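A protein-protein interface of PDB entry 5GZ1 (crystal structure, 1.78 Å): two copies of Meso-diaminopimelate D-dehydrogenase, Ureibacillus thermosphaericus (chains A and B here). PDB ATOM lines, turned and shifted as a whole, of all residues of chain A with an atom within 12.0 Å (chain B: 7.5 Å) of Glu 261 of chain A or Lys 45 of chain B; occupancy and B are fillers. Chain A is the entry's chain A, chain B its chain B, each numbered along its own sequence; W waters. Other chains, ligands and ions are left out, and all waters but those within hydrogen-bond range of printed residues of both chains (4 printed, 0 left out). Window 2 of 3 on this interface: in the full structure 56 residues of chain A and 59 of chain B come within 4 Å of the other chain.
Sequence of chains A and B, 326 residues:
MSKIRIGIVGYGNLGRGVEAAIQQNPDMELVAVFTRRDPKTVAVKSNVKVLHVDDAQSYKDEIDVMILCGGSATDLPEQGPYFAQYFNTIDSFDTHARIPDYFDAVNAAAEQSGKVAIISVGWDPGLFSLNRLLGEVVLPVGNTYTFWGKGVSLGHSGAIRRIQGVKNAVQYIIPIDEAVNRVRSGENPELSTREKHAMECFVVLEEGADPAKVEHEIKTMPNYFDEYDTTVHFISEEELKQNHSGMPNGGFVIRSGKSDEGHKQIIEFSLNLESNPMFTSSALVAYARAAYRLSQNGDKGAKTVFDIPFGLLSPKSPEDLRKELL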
ATOM      1  N   VAL A 138       1.666   7.030  33.121  1.00  0.00           N
ATOM      2  CA  VAL A 138       1.191   7.449  31.767  1.00  0.00           C
ATOM      3  C   VAL A 138      -0.273   7.880  31.718  1.00  0.00           C
ATOM      4  O   VAL A 138      -0.652   8.775  30.937  1.00  0.00           O
ATOM      5  CB  VAL A 138       1.368   6.281  30.816  1.00  0.00           C
ATOM      6  CG1 VAL A 138       0.891   6.610  29.398  1.00  0.00           C
ATOM      7  CG2 VAL A 138       2.853   5.980  30.770  1.00  0.00           C
ATOM      8  N   LEU A 139      -1.100   7.300  32.593  1.00  0.00           N
ATOM      9  CA  LEU A 139      -2.544   7.669  32.631  1.00  0.00           C
ATOM     10  C   LEU A 139      -2.891   8.031  34.082  1.00  0.00           C
ATOM     11  O   LEU A 139      -3.475   7.248  34.785  1.00  0.00           O
ATOM     12  CB  LEU A 139      -3.419   6.538  32.119  1.00  0.00           C
ATOM     13  CG  LEU A 139      -3.274   6.167  30.610  1.00  0.00           C
ATOM     14  CD1 LEU A 139      -4.060   4.910  30.238  1.00  0.00           C
ATOM     15  CD2 LEU A 139      -3.682   7.425  29.765  1.00  0.00           C
ATOM     16  N   PRO A 140      -2.484   9.231  34.493  1.00  0.00           N
ATOM     17  CA  PRO A 140      -2.653   9.543  35.922  1.00  0.00           C
ATOM     18  C   PRO A 140      -4.076   9.668  36.395  1.00  0.00           C
ATOM     19  O   PRO A 140      -4.307   9.595  37.621  1.00  0.00           O
ATOM     20  CB  PRO A 140      -1.932  10.889  36.094  1.00  0.00           C
ATOM     21  CG  PRO A 140      -1.439  11.309  34.736  1.00  0.00           C
ATOM     22  CD  PRO A 140      -1.599  10.175  33.826  1.00  0.00           C
ATOM     23  N   VAL A 141      -4.997   9.894  35.494  1.00  0.00           N
ATOM     24  CA  VAL A 141      -6.395   9.922  35.813  1.00  0.00           C
ATOM     25  C   VAL A 141      -6.999   8.677  35.294  1.00  0.00           C
ATOM     26  O   VAL A 141      -7.202   8.488  34.024  1.00  0.00           O
ATOM     27  CB  VAL A 141      -7.099  11.183  35.248  1.00  0.00           C
ATOM     28  CG1 VAL A 141      -8.626  11.123  35.390  1.00  0.00           C
ATOM     29  CG2 VAL A 141      -6.418  12.450  35.710  1.00  0.00           C
ATOM     30  N   GLY A 142      -7.302   7.752  36.232  1.00  0.00           N
ATOM     31  CA  GLY A 142      -7.885   6.465  35.818  1.00  0.00           C
ATOM     32  C   GLY A 142      -7.871   5.462  36.949  1.00  0.00           C
ATOM     33  O   GLY A 142      -7.647   5.835  38.089  1.00  0.00           O
ATOM     34  N   GLY A 257      -7.923   4.620  31.714  1.00  0.00           N
ATOM     35  CA  GLY A 257      -7.833   6.021  31.999  1.00  0.00           C
ATOM     36  C   GLY A 257      -8.446   6.952  30.980  1.00  0.00           C
ATOM     37  O   GLY A 257      -9.014   6.536  30.037  1.00  0.00           O
ATOM     38  N   LYS A 258      -8.297   8.240  31.226  1.00  0.00           N
ATOM     39  CA  LYS A 258      -8.865   9.261  30.376  1.00  0.00           C
ATOM     40  C   LYS A 258      -7.894  10.394  30.117  1.00  0.00           C
ATOM     41  O   LYS A 258      -7.201  10.794  30.987  1.00  0.00           O
ATOM     42  CB  LYS A 258     -10.119   9.834  31.025  1.00  0.00           C
ATOM     43  CG  LYS A 258     -11.283   8.892  30.998  1.00  0.00           C
ATOM     44  CD  LYS A 258     -12.404   9.411  31.854  1.00  0.00           C
ATOM     45  CE  LYS A 258     -13.757   9.012  31.313  1.00  0.00           C
ATOM     46  NZ  LYS A 258     -13.809   7.667  30.703  1.00  0.00           N
ATOM     47  N   SER A 259      -7.875  10.914  28.905  1.00  0.00           N
ATOM     48  CA  SER A 259      -7.134  12.119  28.634  1.00  0.00           C
ATOM     49  C   SER A 259      -7.882  13.282  29.275  1.00  0.00           C
ATOM     50  O   SER A 259      -8.993  13.139  29.639  1.00  0.00           O
ATOM     51  CB  SER A 259      -7.033  12.372  27.146  1.00  0.00           C
ATOM     52  OG  SER A 259      -8.242  12.867  26.629  1.00  0.00           O
ATOM     53  N   ASP A 260      -7.266  14.443  29.328  1.00  0.00           N
ATOM     54  CA  ASP A 260      -7.929  15.615  29.891  1.00  0.00           C
ATOM     55  C   ASP A 260      -9.126  16.094  29.085  1.00  0.00           C
ATOM     56  O   ASP A 260      -9.857  16.944  29.527  1.00  0.00           O
ATOM     57  CB  ASP A 260      -6.956  16.765  30.111  1.00  0.00           C
ATOM     58  CG  ASP A 260      -7.465  17.763  31.135  1.00  0.00           C
ATOM     59  OD1 ASP A 260      -7.763  17.367  32.263  1.00  0.00           O
ATOM     60  OD2 ASP A 260      -7.575  18.925  30.788  1.00  0.00           O
ATOM     61  N   GLU A 261      -9.312  15.521  27.909  1.00  0.00           N
ATOM     62  CA  GLU A 261     -10.420  15.842  27.036  1.00  0.00           C
ATOM     63  C   GLU A 261     -11.421  14.691  26.926  1.00  0.00           C
ATOM     64  O   GLU A 261     -12.310  14.719  26.106  1.00  0.00           O
ATOM     65  CB  GLU A 261      -9.911  16.240  25.662  1.00  0.00           C
ATOM     66  CG  GLU A 261      -8.994  17.427  25.699  1.00  0.00           C
ATOM     67  CD  GLU A 261      -9.728  18.736  25.857  1.00  0.00           C
ATOM     68  OE1 GLU A 261     -10.912  18.815  25.517  1.00  0.00           O
ATOM     69  OE2 GLU A 261      -9.105  19.697  26.300  1.00  0.00           O
ATOM     70  N   GLY A 262     -11.255  13.686  27.776  1.00  0.00           N
ATOM     71  CA  GLY A 262     -12.220  12.628  27.904  1.00  0.00           C
ATOM     72  C   GLY A 262     -12.011  11.370  27.096  1.00  0.00           C
ATOM     73  O   GLY A 262     -12.823  10.498  27.161  1.00  0.00           O
ATOM     74  N   HIS A 263     -10.922  11.294  26.345  1.00  0.00           N
ATOM     75  CA  HIS A 263     -10.633  10.103  25.557  1.00  0.00           C
ATOM     76  C   HIS A 263     -10.302   8.917  26.447  1.00  0.00           C
ATOM     77  O   HIS A 263      -9.511   9.045  27.312  1.00  0.00           O
ATOM     78  CB  HIS A 263      -9.458  10.342  24.620  1.00  0.00           C
ATOM     79  CG  HIS A 263      -9.612  11.515  23.705  1.00  0.00           C
ATOM     80  ND1 HIS A 263      -8.897  12.673  23.857  1.00  0.00           N
ATOM     81  CD2 HIS A 263     -10.334  11.673  22.580  1.00  0.00           C
ATOM     82  CE1 HIS A 263      -9.200  13.510  22.892  1.00  0.00           C
ATOM     83  NE2 HIS A 263     -10.065  12.923  22.099  1.00  0.00           N
ATOM     84  N   LYS A 264     -10.934   7.786  26.192  1.00  0.00           N
ATOM     85  CA  LYS A 264     -10.680   6.570  26.917  1.00  0.00           C
ATOM     86  C   LYS A 264      -9.429   5.914  26.412  1.00  0.00           C
ATOM     87  O   LYS A 264      -9.324   5.632  25.262  1.00  0.00           O
ATOM     88  CB  LYS A 264     -11.846   5.604  26.768  1.00  0.00           C
ATOM     89  CG  LYS A 264     -13.107   6.097  27.434  1.00  0.00           C
ATOM     90  CD  LYS A 264     -14.103   4.981  27.633  1.00  0.00           C
ATOM     91  CE  LYS A 264     -15.465   5.502  27.991  1.00  0.00           C
ATOM     92  NZ  LYS A 264     -16.282   4.312  28.272  1.00  0.00           N
ATOM     93  N   GLN A 265      -8.501   5.693  27.314  1.00  0.00           N
ATOM     94  CA  GLN A 265      -7.238   5.068  27.006  1.00  0.00           C
ATOM     95  C   GLN A 265      -7.047   3.821  27.880  1.00  0.00           C
ATOM     96  O   GLN A 265      -7.201   3.898  29.042  1.00  0.00           O
ATOM     97  CB  GLN A 265      -6.096   6.054  27.216  1.00  0.00           C
ATOM     98  CG  GLN A 265      -6.374   7.489  26.839  1.00  0.00           C
ATOM     99  CD  GLN A 265      -6.085   7.789  25.382  1.00  0.00           C
ATOM    100  OE1 GLN A 265      -6.544   7.103  24.512  1.00  0.00           O
ATOM    101  NE2 GLN A 265      -5.332   8.815  25.139  1.00  0.00           N
ATOM    102  N   TYR B  11       3.172  23.413  18.424  1.00  0.00           N
ATOM    103  CA  TYR B  11       1.820  23.412  18.938  1.00  0.00           C
ATOM    104  C   TYR B  11       0.845  22.758  17.982  1.00  0.00           C
ATOM    105  O   TYR B  11      -0.361  23.165  17.894  1.00  0.00           O
ATOM    106  CB  TYR B  11       1.349  24.818  19.383  1.00  0.00           C
ATOM    107  CG  TYR B  11       0.205  24.888  20.343  1.00  0.00           C
ATOM    108  CD1 TYR B  11       0.235  24.269  21.611  1.00  0.00           C
ATOM    109  CD2 TYR B  11      -0.955  25.483  19.985  1.00  0.00           C
ATOM    110  CE1 TYR B  11      -0.853  24.380  22.465  1.00  0.00           C
ATOM    111  CE2 TYR B  11      -2.038  25.530  20.823  1.00  0.00           C
ATOM    112  CZ  TYR B  11      -1.982  24.942  22.076  1.00  0.00           C
ATOM    113  OH  TYR B  11      -3.115  24.982  22.901  1.00  0.00           O
ATOM    114  N   ARG B  16      -0.491  20.215  21.761  1.00  0.00           N
ATOM    115  CA  ARG B  16      -1.762  20.328  22.418  1.00  0.00           C
ATOM    116  C   ARG B  16      -2.016  19.239  23.434  1.00  0.00           C
ATOM    117  O   ARG B  16      -2.568  19.473  24.482  1.00  0.00           O
ATOM    118  CB  ARG B  16      -2.903  20.312  21.370  1.00  0.00           C
ATOM    119  CG  ARG B  16      -3.056  21.612  20.586  1.00  0.00           C
ATOM    120  CD  ARG B  16      -4.354  21.664  19.723  1.00  0.00           C
ATOM    121  NE  ARG B  16      -4.426  20.726  18.583  1.00  0.00           N
ATOM    122  CZ  ARG B  16      -3.841  20.912  17.406  1.00  0.00           C
ATOM    123  NH1 ARG B  16      -3.016  21.955  17.157  1.00  0.00           N
ATOM    124  NH2 ARG B  16      -4.019  20.028  16.502  1.00  0.00           N
ATOM    125  N   GLU B  19       0.124  19.971  26.618  1.00  0.00           N
ATOM    126  CA  GLU B  19      -0.655  20.931  27.399  1.00  0.00           C
ATOM    127  C   GLU B  19      -1.749  20.304  28.214  1.00  0.00           C
ATOM    128  O   GLU B  19      -1.977  20.620  29.384  1.00  0.00           O
ATOM    129  CB  GLU B  19      -1.129  22.051  26.434  1.00  0.00           C
ATOM    130  CG  GLU B  19      -1.984  23.134  27.087  1.00  0.00           C
ATOM    131  CD  GLU B  19      -2.430  24.139  25.997  1.00  0.00           C
ATOM    132  OE1 GLU B  19      -2.224  25.341  26.205  1.00  0.00           O
ATOM    133  OE2 GLU B  19      -3.001  23.702  24.965  1.00  0.00           O
ATOM    134  N   ALA B  20      -2.524  19.437  27.578  1.00  0.00           N
ATOM    135  CA  ALA B  20      -3.576  18.731  28.240  1.00  0.00           C
ATOM    136  C   ALA B  20      -3.031  17.828  29.376  1.00  0.00           C
ATOM    137  O   ALA B  20      -3.616  17.784  30.476  1.00  0.00           O
ATOM    138  CB  ALA B  20      -4.361  17.894  27.254  1.00  0.00           C
ATOM    139  N   GLN B  23      -2.302  19.355  32.704  1.00  0.00           N
ATOM    140  CA  GLN B  23      -3.478  19.537  33.575  1.00  0.00           C
ATOM    141  C   GLN B  23      -3.660  18.380  34.508  1.00  0.00           C
ATOM    142  O   GLN B  23      -4.268  18.552  35.553  1.00  0.00           O
ATOM    143  CB  GLN B  23      -4.768  19.674  32.827  1.00  0.00           C
ATOM    144  CG  GLN B  23      -4.852  20.927  32.042  1.00  0.00           C
ATOM    145  CD  GLN B  23      -4.802  22.120  32.997  1.00  0.00           C
ATOM    146  OE1 GLN B  23      -3.862  22.885  32.936  1.00  0.00           O
ATOM    147  NE2 GLN B  23      -5.783  22.219  33.936  1.00  0.00           N
ATOM    148  N   GLN B  24      -3.224  17.159  34.125  1.00  0.00           N
ATOM    149  CA  GLN B  24      -3.355  15.977  34.962  1.00  0.00           C
ATOM    150  C   GLN B  24      -2.129  15.632  35.800  1.00  0.00           C
ATOM    151  O   GLN B  24      -2.124  14.572  36.459  1.00  0.00           O
ATOM    152  CB  GLN B  24      -3.585  14.714  34.046  1.00  0.00           C
ATOM    153  CG  GLN B  24      -4.718  14.930  33.071  1.00  0.00           C
ATOM    154  CD  GLN B  24      -5.081  13.686  32.301  1.00  0.00           C
ATOM    155  OE1 GLN B  24      -4.174  13.137  31.659  1.00  0.00           O
ATOM    156  NE2 GLN B  24      -6.347  13.288  32.262  1.00  0.00           N
ATOM    157  N   VAL B  33       5.237  28.159  25.379  1.00  0.00           N
ATOM    158  CA  VAL B  33       5.022  27.389  24.158  1.00  0.00           C
ATOM    159  C   VAL B  33       5.836  28.095  23.107  1.00  0.00           C
ATOM    160  O   VAL B  33       5.700  29.330  23.013  1.00  0.00           O
ATOM    161  CB  VAL B  33       3.574  27.394  23.756  1.00  0.00           C
ATOM    162  CG1 VAL B  33       3.394  26.723  22.404  1.00  0.00           C
ATOM    163  CG2 VAL B  33       2.731  26.565  24.698  1.00  0.00           C
ATOM    164  N   VAL B  42      -0.665  32.445  17.332  1.00  0.00           N
ATOM    165  CA  VAL B  42      -0.938  31.124  17.966  1.00  0.00           C
ATOM    166  C   VAL B  42      -1.836  31.362  19.179  1.00  0.00           C
ATOM    167  O   VAL B  42      -1.433  32.112  20.080  1.00  0.00           O
ATOM    168  CB  VAL B  42       0.371  30.515  18.408  1.00  0.00           C
ATOM    169  CG1 VAL B  42       0.095  29.174  19.044  1.00  0.00           C
ATOM    170  CG2 VAL B  42       1.276  30.364  17.180  1.00  0.00           C
ATOM    171  N   ALA B  43      -2.995  30.720  19.174  1.00  0.00           N
ATOM    172  CA  ALA B  43      -3.919  30.716  20.258  1.00  0.00           C
ATOM    173  C   ALA B  43      -3.744  29.412  21.103  1.00  0.00           C
ATOM    174  O   ALA B  43      -4.074  28.315  20.638  1.00  0.00           O
ATOM    175  CB  ALA B  43      -5.302  30.780  19.768  1.00  0.00           C
ATOM    176  N   VAL B  44      -3.214  29.591  22.305  1.00  0.00           N
ATOM    177  CA  VAL B  44      -2.912  28.482  23.236  1.00  0.00           C
ATOM    178  C   VAL B  44      -4.049  28.366  24.249  1.00  0.00           C
ATOM    179  O   VAL B  44      -4.509  29.325  24.845  1.00  0.00           O
ATOM    180  CB  VAL B  44      -1.526  28.811  23.890  1.00  0.00           C
ATOM    181  CG1 VAL B  44      -1.303  28.094  25.170  1.00  0.00           C
ATOM    182  CG2 VAL B  44      -0.448  28.373  22.916  1.00  0.00           C
ATOM    183  N   LYS B  45      -4.533  27.186  24.413  1.00  0.00           N
ATOM    184  CA  LYS B  45      -5.708  26.930  25.253  1.00  0.00           C
ATOM    185  C   LYS B  45      -5.460  27.329  26.684  1.00  0.00           C
ATOM    186  O   LYS B  45      -6.301  27.913  27.298  1.00  0.00           O
ATOM    187  CB  LYS B  45      -6.089  25.499  25.151  1.00  0.00           C
ATOM    188  CG  LYS B  45      -7.273  25.132  26.049  1.00  0.00           C
ATOM    189  CD  LYS B  45      -7.796  23.733  25.764  1.00  0.00           C
ATOM    190  CE  LYS B  45      -9.280  23.746  26.113  1.00  0.00           C
ATOM    191  NZ  LYS B  45      -9.837  22.378  26.194  1.00  0.00           N
ATOM    192  N   SER B  46      -4.274  27.160  27.188  1.00  0.00           N
ATOM    193  CA  SER B  46      -4.010  27.379  28.590  1.00  0.00           C
ATOM    194  C   SER B  46      -3.617  28.814  28.829  1.00  0.00           C
ATOM    195  O   SER B  46      -3.400  29.187  29.985  1.00  0.00           O
ATOM    196  CB  SER B  46      -2.833  26.494  29.066  1.00  0.00           C
ATOM    197  OG  SER B  46      -1.672  26.766  28.285  1.00  0.00           O
ATOM    198  N   ASN B  47      -3.474  29.616  27.757  1.00  0.00           N
ATOM    199  CA  ASN B  47      -3.118  31.065  27.900  1.00  0.00           C
ATOM    200  C   ASN B  47      -1.758  31.371  28.453  1.00  0.00           C
ATOM    201  O   ASN B  47      -1.528  32.410  29.007  1.00  0.00           O
ATOM    202  CB  ASN B  47      -4.140  31.798  28.760  1.00  0.00           C
ATOM    203  CG  ASN B  47      -5.461  31.860  28.082  1.00  0.00           C
ATOM    204  OD1 ASN B  47      -5.548  32.395  26.979  1.00  0.00           O
ATOM    205  ND2 ASN B  47      -6.476  31.260  28.679  1.00  0.00           N
ATOM    206  N   VAL B  48      -0.826  30.459  28.256  1.00  0.00           N
ATOM    207  CA  VAL B  48       0.500  30.647  28.689  1.00  0.00           C
ATOM    208  C   VAL B  48       1.164  31.464  27.592  1.00  0.00           C
ATOM    209  O   VAL B  48       0.627  31.503  26.497  1.00  0.00           O
ATOM    210  CB  VAL B  48       1.068  29.218  28.839  1.00  0.00           C
ATOM    211  CG1 VAL B  48       2.505  29.114  28.435  1.00  0.00           C
ATOM    212  CG2 VAL B  48       0.734  28.694  30.234  1.00  0.00           C
ATOM    213  N   GLU B 274      -8.357   5.791  22.400  1.00  0.00           N
ATOM    214  CA  GLU B 274      -9.183   6.769  21.664  1.00  0.00           C
ATOM    215  C   GLU B 274      -8.416   7.929  21.099  1.00  0.00           C
ATOM    216  O   GLU B 274      -8.824   8.509  20.064  1.00  0.00           O
ATOM    217  CB  GLU B 274     -10.339   7.221  22.543  1.00  0.00           C
ATOM    218  CG  GLU B 274     -11.402   6.127  22.674  1.00  0.00           C
ATOM    219  CD  GLU B 274     -12.730   6.678  23.271  1.00  0.00           C
ATOM    220  OE1 GLU B 274     -13.759   5.935  23.076  1.00  0.00           O
ATOM    221  OE2 GLU B 274     -12.749   7.847  23.861  1.00  0.00           O
ATOM    222  N   MET B 278      -2.925  12.271  22.395  1.00  0.00           N
ATOM    223  CA  MET B 278      -3.097  12.500  23.835  1.00  0.00           C
ATOM    224  C   MET B 278      -2.348  11.458  24.670  1.00  0.00           C
ATOM    225  O   MET B 278      -1.853  11.764  25.739  1.00  0.00           O
ATOM    226  CB  MET B 278      -4.549  12.512  24.182  1.00  0.00           C
ATOM    227  CG  MET B 278      -5.187  13.705  23.561  1.00  0.00           C
ATOM    228  SD  MET B 278      -5.111  15.084  24.761  1.00  0.00           S
ATOM    229  CE  MET B 278      -5.613  16.455  23.669  1.00  0.00           C
HETATM  230  O   HOH W   1      -8.260  14.996  33.503  1.00  0.00           O
HETATM  231  O   HOH W   2      -8.436  20.957  32.639  1.00  0.00           O
HETATM  232  O   HOH W   3      -4.460  14.447  28.892  1.00  0.00           O
HETATM  233  O   HOH W   4      -3.988  10.337  27.410  1.00  0.00           O
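The side-chain amide nitrogen of Gln 24 of chain B sits at hydrogen-bond distance from the backbone carbonyl oxygen of Lys 258 of chain A. The backbone NH (N) of Asp 260 of chain A lies close to the side-chain amide nitrogen (NE2) of Gln 24 of chain B, 3.3 Å away. NZ of Lys 45 of chain B is in salt-bridge range of OE2 of Glu 261 of chain A. The backbone NH of Lys 264 of chain A is in hydrogen-bond range of the side-chain carboxylate of Glu 274 of chain B (3.0 Å). The side-chain amide oxygen (OE1) of Gln 265 of chain A is in hydrogen-bond range of the backbone NH (N) of Glu 274 of chain B, at 3.1 Å.
The backbone carbonyl oxygen (O) of Val 141 of chain A lies within hydrogen-bond range of the backbone NH (N) of Lys 258 of chain A, 3.0 Å away. N of Glu 261 of chain A sits close to OG of Ser 259 of chain A, 3.1 Å away. The side-chain hydroxyl of Ser 259 of chain A lies within hydrogen-bond range of the backbone NH of Gly 262 of chain A (3.3 Å). OG of Ser 259 of chain A is in hydrogen-bond range of ND1 of His 263 of chain A (2.9 Å). N of Lys 45 of chain B is in hydrogen-bond range of OH of Tyr 11 of chain B (3.0 Å). The side-chain carboxylate of Glu 19 of chain B is in hydrogen-bond range of the backbone NH of Lys 45 of chain B.
Among the printed residues, pairs that only touch across the chains: Pro 140 of chain A with Gln 24 of chain B, Val 141 of chain A with Gln 24 of chain B, Ser 259 of chain A with Gln 24 of chain B, Ser 259 of chain A with Met 278 of chain B, Asp 260 of chain A with Ala 20 of chain B, Asp 260 of chain A with Gln 23 of chain B, His 263 of chain A with Glu 274 of chain B, His 263 of chain A with Met 278 of chain B and Gln 265 of chain A with Met 278 of chain B.
Of the printed residues of chain B, Pro 140 of chain A touches Gln 24 (3.7 Å). Gly 142 of chain A touches none of the printed residues of chain B. Printed residues of chain B within 4 Å of Lys 258 of chain A: Gln 24. Glu 261 of chain A touches just one residue of chain B: Lys 45. Glu 19 of chain B touches none of the printed residues of chain A. Ala 20 of chain B touches one residue of chain A. No residue of chain A comes within 4 Å of Ala 43 of chain B. No residue of chain A comes within 4 Å of Val 44 of chain B. Of chain A, only Glu 261 comes within 4 Å of Lys 45 of chain B. No residue of chain A comes within 4 Å of Ser 46 of chain B. No residue of chain A comes within 4 Å of Asn 47 of chain B. Printed residues of chain A within 4 Å of Met 278 of chain B: Ser 259, His 263 and Gln 265. The nearest residue of chain A that does not touch Lys 45 of chain B is Asp 260 of chain A (6.2 Å).
Of the 16 printed residues of chain B, 6 touch a printed residue of chain A. Hydrophobic or aromatic side chains of chain B that line the printed part of chain A: Met 278. Among the printed residues, 14 pairs touch across the chains.
No position is printed for both chains.
Water W1 lies within hydrogen-bond range of the side-chain carboxylate of Asp 260 of chain A (2.7 Å) and the side-chain amide nitrogen of Gln 24 of chain B (2.8 Å). Water W3 lies within hydrogen-bond range of N of Asp 260 of chain A (2.8 Å) and OE1 of Gln 24 of chain B (3.1 Å). Water W2 lies within hydrogen-bond range of OD2 of Asp 260 of chain A (2.9 Å) and NE2 of Gln 23 of chain B (3.2 Å). Water W4 lies within hydrogen-bond range of the side-chain amide nitrogen of Gln 265 of chain A (3.0 Å) and the backbone carbonyl oxygen of Met 278 of chain B (3.1 Å).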
